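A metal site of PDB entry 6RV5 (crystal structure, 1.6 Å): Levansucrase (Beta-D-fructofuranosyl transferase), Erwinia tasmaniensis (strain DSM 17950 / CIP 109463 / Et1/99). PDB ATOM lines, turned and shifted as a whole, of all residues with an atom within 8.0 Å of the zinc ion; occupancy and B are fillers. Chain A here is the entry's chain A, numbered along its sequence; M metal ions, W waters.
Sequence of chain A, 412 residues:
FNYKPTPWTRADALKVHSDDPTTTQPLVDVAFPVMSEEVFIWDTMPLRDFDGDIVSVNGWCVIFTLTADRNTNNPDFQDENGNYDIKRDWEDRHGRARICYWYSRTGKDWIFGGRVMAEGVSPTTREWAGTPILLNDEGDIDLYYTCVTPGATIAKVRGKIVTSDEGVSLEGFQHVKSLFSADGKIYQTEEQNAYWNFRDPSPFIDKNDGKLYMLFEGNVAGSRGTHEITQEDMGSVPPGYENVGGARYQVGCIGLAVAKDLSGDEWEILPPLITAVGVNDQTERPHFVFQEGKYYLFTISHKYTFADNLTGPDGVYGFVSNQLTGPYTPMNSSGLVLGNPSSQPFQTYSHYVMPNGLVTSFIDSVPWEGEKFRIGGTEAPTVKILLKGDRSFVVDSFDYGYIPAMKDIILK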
ATOM      1  N   ARG A  48      28.516   7.456   9.908  1.00  0.00           N
ATOM      2  CA  ARG A  48      27.158   7.809   9.525  1.00  0.00           C
ATOM      3  C   ARG A  48      26.197   7.810  10.740  1.00  0.00           C
ATOM      4  O   ARG A  48      26.571   7.336  11.811  1.00  0.00           O
ATOM      5  CB  ARG A  48      26.782   6.937   8.328  1.00  0.00           C
ATOM      6  CG  ARG A  48      26.476   5.480   8.620  1.00  0.00           C
ATOM      7  CD  ARG A  48      25.729   4.997   7.376  1.00  0.00           C
ATOM      8  NE  ARG A  48      25.277   3.604   7.377  1.00  0.00           N
ATOM      9  CZ  ARG A  48      24.062   3.142   7.705  1.00  0.00           C
ATOM     10  NH1 ARG A  48      23.092   3.957   8.115  1.00  0.00           N
ATOM     11  NH2 ARG A  48      23.827   1.831   7.630  1.00  0.00           N
ATOM     12  N   ASP A  49      24.994   8.394  10.531  1.00  0.00           N
ATOM     13  CA  ASP A  49      23.935   8.353  11.543  1.00  0.00           C
ATOM     14  C   ASP A  49      22.997   7.202  11.189  1.00  0.00           C
ATOM     15  O   ASP A  49      23.183   6.468  10.214  1.00  0.00           O
ATOM     16  CB  ASP A  49      23.300   9.731  11.732  1.00  0.00           C
ATOM     17  CG  ASP A  49      22.457  10.207  10.580  1.00  0.00           C
ATOM     18  OD1 ASP A  49      22.232   9.410   9.628  1.00  0.00           O
ATOM     19  OD2 ASP A  49      22.163  11.407  10.617  1.00  0.00           O
ATOM     20  N   PHE A  50      21.974   7.026  11.996  1.00  0.00           N
ATOM     21  CA  PHE A  50      21.027   5.923  11.806  1.00  0.00           C
ATOM     22  C   PHE A  50      20.148   6.110  10.549  1.00  0.00           C
ATOM     23  O   PHE A  50      19.498   5.124  10.248  1.00  0.00           O
ATOM     24  CB  PHE A  50      20.200   5.736  13.096  1.00  0.00           C
ATOM     25  CG  PHE A  50      20.837   4.852  14.141  1.00  0.00           C
ATOM     26  CD1 PHE A  50      21.165   3.523  13.866  1.00  0.00           C
ATOM     27  CD2 PHE A  50      21.076   5.313  15.416  1.00  0.00           C
ATOM     28  CE1 PHE A  50      21.755   2.715  14.827  1.00  0.00           C
ATOM     29  CE2 PHE A  50      21.621   4.499  16.383  1.00  0.00           C
ATOM     30  CZ  PHE A  50      21.949   3.198  16.092  1.00  0.00           C
ATOM     31  N   ASP A  51      20.248   7.192   9.782  1.00  0.00           N
ATOM     32  CA  ASP A  51      19.481   7.209   8.523  1.00  0.00           C
ATOM     33  C   ASP A  51      20.400   7.053   7.311  1.00  0.00           C
ATOM     34  O   ASP A  51      19.891   6.859   6.223  1.00  0.00           O
ATOM     35  CB  ASP A  51      18.522   8.391   8.433  1.00  0.00           C
ATOM     36  CG  ASP A  51      19.280   9.677   8.550  1.00  0.00           C
ATOM     37  OD1 ASP A  51      20.026   9.892   7.653  1.00  0.00           O
ATOM     38  OD2 ASP A  51      19.113  10.406   9.528  1.00  0.00           O
ATOM     39  N   GLY A  52      21.715   7.083   7.481  1.00  0.00           N
ATOM     40  CA  GLY A  52      22.573   6.856   6.315  1.00  0.00           C
ATOM     41  C   GLY A  52      23.339   8.106   5.977  1.00  0.00           C
ATOM     42  O   GLY A  52      24.307   7.997   5.268  1.00  0.00           O
ATOM     43  N   ASP A  53      22.922   9.241   6.543  1.00  0.00           N
ATOM     44  CA  ASP A  53      23.691  10.488   6.339  1.00  0.00           C
ATOM     45  C   ASP A  53      25.126  10.294   6.817  1.00  0.00           C
ATOM     46  O   ASP A  53      25.331   9.762   7.864  1.00  0.00           O
ATOM     47  CB  ASP A  53      23.206  11.617   7.236  1.00  0.00           C
ATOM     48  CG  ASP A  53      21.945  12.308   6.772  1.00  0.00           C
ATOM     49  OD1 ASP A  53      21.573  12.106   5.623  1.00  0.00           O
ATOM     50  OD2 ASP A  53      21.320  12.925   7.621  1.00  0.00           O
ATOM     51  N   ILE A  54      26.049  10.765   6.011  1.00  0.00           N
ATOM     52  CA  ILE A  54      27.476  10.811   6.380  1.00  0.00           C
ATOM     53  C   ILE A  54      27.656  12.038   7.296  1.00  0.00           C
ATOM     54  O   ILE A  54      27.252  13.162   6.940  1.00  0.00           O
ATOM     55  CB  ILE A  54      28.366  10.894   5.160  1.00  0.00           C
ATOM     56  CG1 ILE A  54      27.999   9.820   4.116  1.00  0.00           C
ATOM     57  CG2 ILE A  54      29.844  10.817   5.581  1.00  0.00           C
ATOM     58  CD1 ILE A  54      27.833   8.397   4.649  1.00  0.00           C
ATOM     59  N   VAL A  55      28.254  11.838   8.462  1.00  0.00           N
ATOM     60  CA  VAL A  55      28.394  12.900   9.465  1.00  0.00           C
ATOM     61  C   VAL A  55      29.872  13.117   9.809  1.00  0.00           C
ATOM     62  O   VAL A  55      30.619  12.135   9.963  1.00  0.00           O
ATOM     63  CB  VAL A  55      27.595  12.577  10.744  1.00  0.00           C
ATOM     64  CG1 VAL A  55      26.114  12.605  10.487  1.00  0.00           C
ATOM     65  CG2 VAL A  55      28.028  11.264  11.387  1.00  0.00           C
ATOM     66  N   LYS A 207      11.882   5.240  10.168  1.00  0.00           N
ATOM     67  CA  LYS A 207      10.938   6.161  10.860  1.00  0.00           C
ATOM     68  C   LYS A 207       9.476   5.714  10.706  1.00  0.00           C
ATOM     69  O   LYS A 207       8.643   6.136  11.530  1.00  0.00           O
ATOM     70  CB  LYS A 207      11.131   7.591  10.361  1.00  0.00           C
ATOM     71  CG  LYS A 207      12.440   8.232  10.805  1.00  0.00           C
ATOM     72  CD  LYS A 207      12.591   9.657  10.403  1.00  0.00           C
ATOM     73  CE  LYS A 207      14.015  10.148  10.492  1.00  0.00           C
ATOM     74  NZ  LYS A 207      14.543  10.127  11.882  1.00  0.00           N
ATOM     75  N   MET A 406      27.760  14.973   4.914  1.00  0.00           N
ATOM     76  CA  MET A 406      26.491  15.628   4.549  1.00  0.00           C
ATOM     77  C   MET A 406      26.038  16.584   5.627  1.00  0.00           C
ATOM     78  O   MET A 406      25.370  17.599   5.283  1.00  0.00           O
ATOM     79  CB  MET A 406      25.419  14.560   4.344  1.00  0.00           C
ATOM     80  CG  MET A 406      25.742  13.704   3.104  1.00  0.00           C
ATOM     81  SD  MET A 406      24.753  12.252   2.964  1.00  0.00           S
ATOM     82  CE  MET A 406      23.172  13.103   2.793  1.00  0.00           C
ATOM     83  N   LYS A 407      26.328  16.245   6.876  1.00  0.00           N
ATOM     84  CA  LYS A 407      26.117  17.234   7.953  1.00  0.00           C
ATOM     85  C   LYS A 407      27.135  17.056   9.055  1.00  0.00           C
ATOM     86  O   LYS A 407      27.810  16.004   9.160  1.00  0.00           O
ATOM     87  CB  LYS A 407      24.685  17.214   8.484  1.00  0.00           C
ATOM     88  CG  LYS A 407      24.251  15.965   9.222  1.00  0.00           C
ATOM     89  CD  LYS A 407      23.387  16.344  10.409  1.00  0.00           C
ATOM     90  CE  LYS A 407      22.131  15.511  10.493  1.00  0.00           C
ATOM     91  NZ  LYS A 407      21.816  15.141  11.874  1.00  0.00           N
ATOM     92  N   ILE A 409      28.085  17.416  13.007  1.00  0.00           N
ATOM     93  CA  ILE A 409      27.544  17.292  14.379  1.00  0.00           C
ATOM     94  C   ILE A 409      28.485  18.044  15.334  1.00  0.00           C
ATOM     95  O   ILE A 409      29.716  17.711  15.375  1.00  0.00           O
ATOM     96  CB  ILE A 409      27.389  15.833  14.756  1.00  0.00           C
ATOM     97  CG1 ILE A 409      26.542  15.124  13.704  1.00  0.00           C
ATOM     98  CG2 ILE A 409      26.837  15.710  16.178  1.00  0.00           C
ATOM     99  CD1 ILE A 409      25.104  15.614  13.592  1.00  0.00           C
HETATM  100 ZN    ZN M   1      20.626  11.936   9.475  1.00  0.00          ZN
HETATM  101  O   HOH W   1      19.741  13.492  10.518  1.00  0.00           O
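OD2 of Asp 49 is bound to the zinc ion (2.0 Å).
The zinc ion is bound by water W1, at 2.1 Å.
The zinc ion is bound by the side-chain carboxylate (OD2) of Asp 51 (2.2 Å).
The zinc ion is bound by OD2 of Asp 53, 2.2 Å away.
The zinc ion has four donor atoms within binding distance.
Slightly farther from the zinc ion lies the side-chain carboxylate (OD1) of Asp 51 (2.8 Å).
Of the 12 residues printed, 3 come within 4 Å of the zinc ion.
The nearest printed residue that does not touch the zinc ion is Lys 407 (4.01 Å).
OD2 of Asp 49 lies close to NZ of Lys 407 (3.96 Å).
The backbone NH (N) of Gly 52 sits at hydrogen-bond distance from the side-chain carboxylate (OD1) of Asp 49.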
